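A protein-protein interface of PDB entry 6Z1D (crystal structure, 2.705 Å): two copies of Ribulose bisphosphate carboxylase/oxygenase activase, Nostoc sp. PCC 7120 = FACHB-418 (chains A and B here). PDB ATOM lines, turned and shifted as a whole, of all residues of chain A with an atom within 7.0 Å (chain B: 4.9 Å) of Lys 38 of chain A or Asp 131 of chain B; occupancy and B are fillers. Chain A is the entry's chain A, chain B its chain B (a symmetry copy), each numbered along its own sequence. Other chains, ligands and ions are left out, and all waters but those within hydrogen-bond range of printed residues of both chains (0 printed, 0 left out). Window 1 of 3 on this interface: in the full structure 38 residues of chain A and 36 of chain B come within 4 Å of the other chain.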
ATOM      1  N   GLY A  36      33.681   6.833 -32.791  1.00  0.00           N
ATOM      2  CA  GLY A  36      32.961   5.732 -33.363  1.00  0.00           C
ATOM      3  C   GLY A  36      31.702   5.539 -32.572  1.00  0.00           C
ATOM      4  O   GLY A  36      31.433   6.255 -31.605  1.00  0.00           O
ATOM      5  N   ARG A  37      30.957   4.528 -32.972  1.00  0.00           N
ATOM      6  CA  ARG A  37      29.621   4.306 -32.466  1.00  0.00           C
ATOM      7  C   ARG A  37      29.618   3.693 -31.059  1.00  0.00           C
ATOM      8  O   ARG A  37      30.637   3.184 -30.587  1.00  0.00           O
ATOM      9  CB  ARG A  37      28.912   3.411 -33.468  1.00  0.00           C
ATOM     10  CG  ARG A  37      27.511   3.054 -33.129  1.00  0.00           C
ATOM     11  CD  ARG A  37      26.831   2.455 -34.322  1.00  0.00           C
ATOM     12  NE  ARG A  37      27.186   1.046 -34.479  1.00  0.00           N
ATOM     13  CZ  ARG A  37      26.435   0.153 -35.123  1.00  0.00           C
ATOM     14  NH1 ARG A  37      26.830  -1.110 -35.223  1.00  0.00           N
ATOM     15  NH2 ARG A  37      25.279   0.526 -35.665  1.00  0.00           N
ATOM     16  N   LYS A  38      28.471   3.764 -30.390  1.00  0.00           N
ATOM     17  CA  LYS A  38      28.326   3.266 -29.016  1.00  0.00           C
ATOM     18  C   LYS A  38      28.049   1.759 -29.046  1.00  0.00           C
ATOM     19  O   LYS A  38      27.403   1.252 -29.966  1.00  0.00           O
ATOM     20  CB  LYS A  38      27.200   4.039 -28.275  1.00  0.00           C
ATOM     21  CG  LYS A  38      26.245   3.203 -27.366  1.00  0.00           C
ATOM     22  CD  LYS A  38      24.971   3.978 -26.932  1.00  0.00           C
ATOM     23  CE  LYS A  38      23.683   3.229 -27.320  1.00  0.00           C
ATOM     24  NZ  LYS A  38      22.595   3.270 -26.286  1.00  0.00           N
ATOM     25  N   GLY A  39      28.528   1.043 -28.037  1.00  0.00           N
ATOM     26  CA  GLY A  39      28.270  -0.384 -27.935  1.00  0.00           C
ATOM     27  C   GLY A  39      29.260  -1.217 -28.718  1.00  0.00           C
ATOM     28  O   GLY A  39      28.990  -2.370 -29.053  1.00  0.00           O
ATOM     29  N   GLU A  40      30.423  -0.627 -28.980  1.00  0.00           N
ATOM     30  CA  GLU A  40      31.484  -1.292 -29.717  1.00  0.00           C
ATOM     31  C   GLU A  40      32.721  -1.503 -28.850  1.00  0.00           C
ATOM     32  O   GLU A  40      33.758  -1.918 -29.346  1.00  0.00           O
ATOM     33  CB  GLU A  40      31.839  -0.493 -30.970  1.00  0.00           C
ATOM     34  CG  GLU A  40      30.650  -0.194 -31.875  1.00  0.00           C
ATOM     35  CD  GLU A  40      30.149  -1.409 -32.634  1.00  0.00           C
ATOM     36  OE1 GLU A  40      30.482  -2.544 -32.253  1.00  0.00           O
ATOM     37  OE2 GLU A  40      29.418  -1.227 -33.625  1.00  0.00           O
ATOM     38  N   GLY A  41      32.611  -1.220 -27.558  1.00  0.00           N
ATOM     39  CA  GLY A  41      33.657  -1.573 -26.614  1.00  0.00           C
ATOM     40  C   GLY A  41      34.836  -0.610 -26.596  1.00  0.00           C
ATOM     41  O   GLY A  41      35.954  -0.987 -26.253  1.00  0.00           O
ATOM     42  N   LYS A  42      34.595   0.638 -26.974  1.00  0.00           N
ATOM     43  CA  LYS A  42      35.648   1.650 -26.975  1.00  0.00           C
ATOM     44  C   LYS A  42      36.346   1.802 -25.631  1.00  0.00           C
ATOM     45  O   LYS A  42      37.478   1.351 -25.469  1.00  0.00           O
ATOM     46  CB  LYS A  42      35.076   3.007 -27.335  1.00  0.00           C
ATOM     47  CG  LYS A  42      35.455   3.489 -28.691  1.00  0.00           C
ATOM     48  CD  LYS A  42      35.010   4.911 -28.847  1.00  0.00           C
ATOM     49  CE  LYS A  42      33.591   4.972 -29.366  1.00  0.00           C
ATOM     50  NZ  LYS A  42      32.782   5.968 -28.628  1.00  0.00           N
ATOM     51  N   PHE A 109      21.303  11.795 -28.039  1.00  0.00           N
ATOM     52  CA  PHE A 109      21.426  11.677 -26.594  1.00  0.00           C
ATOM     53  C   PHE A 109      21.112  13.027 -25.967  1.00  0.00           C
ATOM     54  O   PHE A 109      21.441  13.281 -24.805  1.00  0.00           O
ATOM     55  CB  PHE A 109      22.842  11.238 -26.229  1.00  0.00           C
ATOM     56  CG  PHE A 109      23.331  10.082 -27.041  1.00  0.00           C
ATOM     57  CD1 PHE A 109      22.798   8.817 -26.855  1.00  0.00           C
ATOM     58  CD2 PHE A 109      24.308  10.260 -27.997  1.00  0.00           C
ATOM     59  CE1 PHE A 109      23.237   7.746 -27.605  1.00  0.00           C
ATOM     60  CE2 PHE A 109      24.754   9.197 -28.751  1.00  0.00           C
ATOM     61  CZ  PHE A 109      24.215   7.934 -28.553  1.00  0.00           C
ATOM     62  N   ASN A 157      31.592  10.158 -29.746  1.00  0.00           N
ATOM     63  CA  ASN A 157      30.965   9.517 -30.888  1.00  0.00           C
ATOM     64  C   ASN A 157      31.485  10.114 -32.190  1.00  0.00           C
ATOM     65  O   ASN A 157      31.707   9.405 -33.173  1.00  0.00           O
ATOM     66  CB  ASN A 157      29.448   9.629 -30.784  1.00  0.00           C
ATOM     67  CG  ASN A 157      28.914   9.012 -29.501  1.00  0.00           C
ATOM     68  OD1 ASN A 157      29.349   7.929 -29.092  1.00  0.00           O
ATOM     69  ND2 ASN A 157      27.985   9.708 -28.846  1.00  0.00           N
ATOM     70  N   SER A 213      26.143  -4.229 -33.290  1.00  0.00           N
ATOM     71  CA  SER A 213      27.265  -3.796 -32.477  1.00  0.00           C
ATOM     72  C   SER A 213      27.720  -4.964 -31.645  1.00  0.00           C
ATOM     73  O   SER A 213      27.031  -5.968 -31.547  1.00  0.00           O
ATOM     74  CB  SER A 213      26.832  -2.688 -31.533  1.00  0.00           C
ATOM     75  OG  SER A 213      25.988  -3.229 -30.535  1.00  0.00           O
ATOM     76  N   ILE A 214      28.881  -4.823 -31.035  1.00  0.00           N
ATOM     77  CA  ILE A 214      29.398  -5.831 -30.131  1.00  0.00           C
ATOM     78  C   ILE A 214      28.404  -6.088 -28.992  1.00  0.00           C
ATOM     79  O   ILE A 214      28.167  -7.233 -28.616  1.00  0.00           O
ATOM     80  CB  ILE A 214      30.786  -5.397 -29.605  1.00  0.00           C
ATOM     81  CG1 ILE A 214      31.800  -5.415 -30.756  1.00  0.00           C
ATOM     82  CG2 ILE A 214      31.257  -6.289 -28.457  1.00  0.00           C
ATOM     83  CD1 ILE A 214      31.982  -6.788 -31.424  1.00  0.00           C
ATOM     84  N   ASP A 215      27.796  -5.028 -28.471  1.00  0.00           N
ATOM     85  CA  ASP A 215      26.830  -5.158 -27.380  1.00  0.00           C
ATOM     86  C   ASP A 215      25.606  -6.014 -27.720  1.00  0.00           C
ATOM     87  O   ASP A 215      25.002  -6.601 -26.836  1.00  0.00           O
ATOM     88  CB  ASP A 215      26.378  -3.773 -26.926  1.00  0.00           C
ATOM     89  CG  ASP A 215      27.308  -3.162 -25.895  1.00  0.00           C
ATOM     90  OD1 ASP A 215      28.433  -3.678 -25.724  1.00  0.00           O
ATOM     91  OD2 ASP A 215      26.912  -2.159 -25.261  1.00  0.00           O
ATOM     92  N   LEU B 126      16.324   7.988 -21.352  1.00  0.00           N
ATOM     93  CA  LEU B 126      16.341   6.576 -20.986  1.00  0.00           C
ATOM     94  C   LEU B 126      17.547   5.877 -21.582  1.00  0.00           C
ATOM     95  O   LEU B 126      18.112   4.986 -20.952  1.00  0.00           O
ATOM     96  CB  LEU B 126      15.046   5.889 -21.411  1.00  0.00           C
ATOM     97  CG  LEU B 126      13.796   6.421 -20.704  1.00  0.00           C
ATOM     98  CD1 LEU B 126      12.558   5.806 -21.313  1.00  0.00           C
ATOM     99  CD2 LEU B 126      13.837   6.152 -19.190  1.00  0.00           C
ATOM    100  N   MET B 127      17.944   6.285 -22.786  1.00  0.00           N
ATOM    101  CA  MET B 127      19.175   5.784 -23.386  1.00  0.00           C
ATOM    102  C   MET B 127      20.371   6.089 -22.484  1.00  0.00           C
ATOM    103  O   MET B 127      21.123   5.187 -22.114  1.00  0.00           O
ATOM    104  CB  MET B 127      19.395   6.387 -24.780  1.00  0.00           C
ATOM    105  CG  MET B 127      18.809   5.544 -25.917  1.00  0.00           C
ATOM    106  SD  MET B 127      18.485   6.414 -27.482  1.00  0.00           S
ATOM    107  CE  MET B 127      20.135   6.815 -28.055  1.00  0.00           C
ATOM    108  N   ASN B 128      20.533   7.355 -22.114  1.00  0.00           N
ATOM    109  CA  ASN B 128      21.670   7.761 -21.296  1.00  0.00           C
ATOM    110  C   ASN B 128      21.686   7.056 -19.949  1.00  0.00           C
ATOM    111  O   ASN B 128      22.737   6.663 -19.460  1.00  0.00           O
ATOM    112  CB  ASN B 128      21.661   9.271 -21.085  1.00  0.00           C
ATOM    113  CG  ASN B 128      21.795  10.033 -22.380  1.00  0.00           C
ATOM    114  OD1 ASN B 128      22.271   9.496 -23.378  1.00  0.00           O
ATOM    115  ND2 ASN B 128      21.371  11.290 -22.373  1.00  0.00           N
ATOM    116  N   ILE B 129      20.526   6.902 -19.337  1.00  0.00           N
ATOM    117  CA  ILE B 129      20.467   6.219 -18.059  1.00  0.00           C
ATOM    118  C   ILE B 129      20.833   4.761 -18.246  1.00  0.00           C
ATOM    119  O   ILE B 129      21.616   4.217 -17.475  1.00  0.00           O
ATOM    120  CB  ILE B 129      19.087   6.344 -17.409  1.00  0.00           C
ATOM    121  CG1 ILE B 129      18.882   7.788 -16.945  1.00  0.00           C
ATOM    122  CG2 ILE B 129      18.965   5.391 -16.231  1.00  0.00           C
ATOM    123  CD1 ILE B 129      17.447   8.146 -16.612  1.00  0.00           C
ATOM    124  N   ALA B 130      20.270   4.128 -19.267  1.00  0.00           N
ATOM    125  CA  ALA B 130      20.524   2.707 -19.511  1.00  0.00           C
ATOM    126  C   ALA B 130      22.002   2.445 -19.818  1.00  0.00           C
ATOM    127  O   ALA B 130      22.533   1.396 -19.459  1.00  0.00           O
ATOM    128  CB  ALA B 130      19.650   2.200 -20.643  1.00  0.00           C
ATOM    129  N   ASP B 131      22.652   3.410 -20.468  1.00  0.00           N
ATOM    130  CA  ASP B 131      24.074   3.315 -20.780  1.00  0.00           C
ATOM    131  C   ASP B 131      24.935   3.237 -19.518  1.00  0.00           C
ATOM    132  O   ASP B 131      25.974   2.586 -19.521  1.00  0.00           O
ATOM    133  CB  ASP B 131      24.525   4.509 -21.621  1.00  0.00           C
ATOM    134  CG  ASP B 131      24.256   4.332 -23.115  1.00  0.00           C
ATOM    135  OD1 ASP B 131      24.236   3.182 -23.617  1.00  0.00           O
ATOM    136  OD2 ASP B 131      24.095   5.368 -23.803  1.00  0.00           O
ATOM    137  N   ASN B 132      24.513   3.916 -18.454  1.00  0.00           N
ATOM    138  CA  ASN B 132      25.224   3.890 -17.169  1.00  0.00           C
ATOM    139  C   ASN B 132      24.254   4.070 -16.013  1.00  0.00           C
ATOM    140  O   ASN B 132      24.138   5.173 -15.477  1.00  0.00           O
ATOM    141  CB  ASN B 132      26.272   5.008 -17.079  1.00  0.00           C
ATOM    142  CG  ASN B 132      27.420   4.820 -18.039  1.00  0.00           C
ATOM    143  OD1 ASN B 132      28.375   4.092 -17.755  1.00  0.00           O
ATOM    144  ND2 ASN B 132      27.349   5.497 -19.181  1.00  0.00           N
ATOM    145  N   PRO B 133      23.570   2.987 -15.607  1.00  0.00           N
ATOM    146  CA  PRO B 133      22.536   3.033 -14.563  1.00  0.00           C
ATOM    147  C   PRO B 133      23.065   3.457 -13.198  1.00  0.00           C
ATOM    148  O   PRO B 133      22.294   3.710 -12.278  1.00  0.00           O
ATOM    149  CB  PRO B 133      22.055   1.579 -14.486  1.00  0.00           C
ATOM    150  CG  PRO B 133      22.517   0.937 -15.738  1.00  0.00           C
ATOM    151  CD  PRO B 133      23.787   1.613 -16.085  1.00  0.00           C
ATOM    152  N   LEU B 166      18.387   0.770 -28.324  1.00  0.00           N
ATOM    153  CA  LEU B 166      18.429   0.249 -26.964  1.00  0.00           C
ATOM    154  C   LEU B 166      18.146  -1.247 -26.926  1.00  0.00           C
ATOM    155  O   LEU B 166      18.823  -2.004 -26.230  1.00  0.00           O
ATOM    156  CB  LEU B 166      17.392   0.954 -26.088  1.00  0.00           C
ATOM    157  CG  LEU B 166      17.754   2.241 -25.360  1.00  0.00           C
ATOM    158  CD1 LEU B 166      16.564   2.721 -24.556  1.00  0.00           C
ATOM    159  CD2 LEU B 166      18.913   2.004 -24.433  1.00  0.00           C
ATOM    160  N   ASP B 169      21.041  -3.335 -28.459  1.00  0.00           N
ATOM    161  CA  ASP B 169      22.258  -3.460 -27.658  1.00  0.00           C
ATOM    162  C   ASP B 169      21.959  -4.035 -26.279  1.00  0.00           C
ATOM    163  O   ASP B 169      22.805  -3.991 -25.385  1.00  0.00           O
ATOM    164  CB  ASP B 169      22.957  -2.109 -27.518  1.00  0.00           C
ATOM    165  CG  ASP B 169      23.507  -1.600 -28.836  1.00  0.00           C
ATOM    166  OD1 ASP B 169      23.409  -2.333 -29.844  1.00  0.00           O
ATOM    167  OD2 ASP B 169      24.051  -0.476 -28.867  1.00  0.00           O
ATOM    168  N   ARG B 171      20.023  -3.091 -23.845  1.00  0.00           N
ATOM    169  CA  ARG B 171      19.783  -2.178 -22.733  1.00  0.00           C
ATOM    170  C   ARG B 171      18.293  -2.036 -22.464  1.00  0.00           C
ATOM    171  O   ARG B 171      17.878  -1.489 -21.448  1.00  0.00           O
ATOM    172  CB  ARG B 171      20.392  -0.817 -23.033  1.00  0.00           C
ATOM    173  CG  ARG B 171      21.788  -0.917 -23.574  1.00  0.00           C
ATOM    174  CD  ARG B 171      22.683   0.149 -23.029  1.00  0.00           C
ATOM    175  NE  ARG B 171      23.902   0.228 -23.819  1.00  0.00           N
ATOM    176  CZ  ARG B 171      25.009  -0.464 -23.578  1.00  0.00           C
ATOM    177  NH1 ARG B 171      26.052  -0.312 -24.375  1.00  0.00           N
ATOM    178  NH2 ARG B 171      25.083  -1.296 -22.548  1.00  0.00           N
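The side-chain carboxylate of Asp 215 of chain A is in salt-bridge range of the guanidinium group of Arg 171 of chain B, at 3.4 Å.
The side-chain amino group (NZ) of Lys 38 of chain A lies within salt-bridge range of the side-chain carboxylate (OD1) of Asp 131 of chain B, at 3.1 Å.
The backbone carbonyl oxygen of Phe 109 of chain A lies within hydrogen-bond range of the side-chain amide nitrogen of Asn 128 of chain B.
The side-chain carboxylate (OD1) of Asp 169 of chain B is in hydrogen-bond range of the side-chain hydroxyl (OG) of Ser 213 of chain A.
The guanidinium group (NE) of Arg 171 of chain B lies within salt-bridge range of the side-chain carboxylate (OD1) of Asp 131 of chain B (3.0 Å).
N of Arg 171 of chain B lies within hydrogen-bond range of O of Leu 166 of chain B.
O of Gly 39 of chain A lies within hydrogen-bond range of N of Asp 215 of chain A (3.0 Å).
The side-chain hydroxyl of Ser 213 of chain A sits close to the backbone NH of Asp 215 of chain A (3.3 Å).
O of Gly 39 of chain A lies close to OG of Ser 213 of chain A.
Among the printed residues, merely in contact across the chains: Phe 109 of chain A with Met 127 of chain B (3.3 Å), Asp 215 of chain A with Asp 169 of chain B (3.7 Å) and Lys 38 of chain A with Asp 169 of chain B (3.9 Å).
Of chain B, only Asp 131 and Asp 169 come within 4 Å of Lys 38 of chain A.
Of chain A, only Lys 38 (3.1 Å) comes within 4 Å of Asp 131 of chain B.
Printed residues of chain A within 4 Å of Asn 128 of chain B: Phe 109 (3.1 Å).
Printed residues of chain A within 4 Å of Arg 171 of chain B: Asp 215.
Of the printed residues of chain B, Asp 215 of chain A touches Asp 169 and Arg 171.
Of the printed residues of chain B, Ser 213 of chain A touches Asp 169.
The nearest residue of chain B that does not touch Lys 38 of chain A is Arg 171 of chain B (4.1 Å).
The nearest residue of chain A that does not touch Asp 131 of chain B is Phe 109 of chain A (4.6 Å).
The nearest printed residue of chain A that does not touch Asn 128 of chain B is Lys 38 of chain A (6.2 Å).
Of the 11 printed residues of chain B, 5 touch a printed residue of chain A.
Along chain B the printed residues that touch a printed residue of chain A span positions 127 to 171.
Hydrophobic or aromatic side chains of chain A within 4 Å of the printed part of chain B: Phe 109.
Along chain A the printed residues that touch a printed residue of chain B span positions 38 to 215.
No position is printed for both chains.
Of the 7 pairs that touch across the chains among the printed residues, none has its exchanged pair printed and touching as well.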
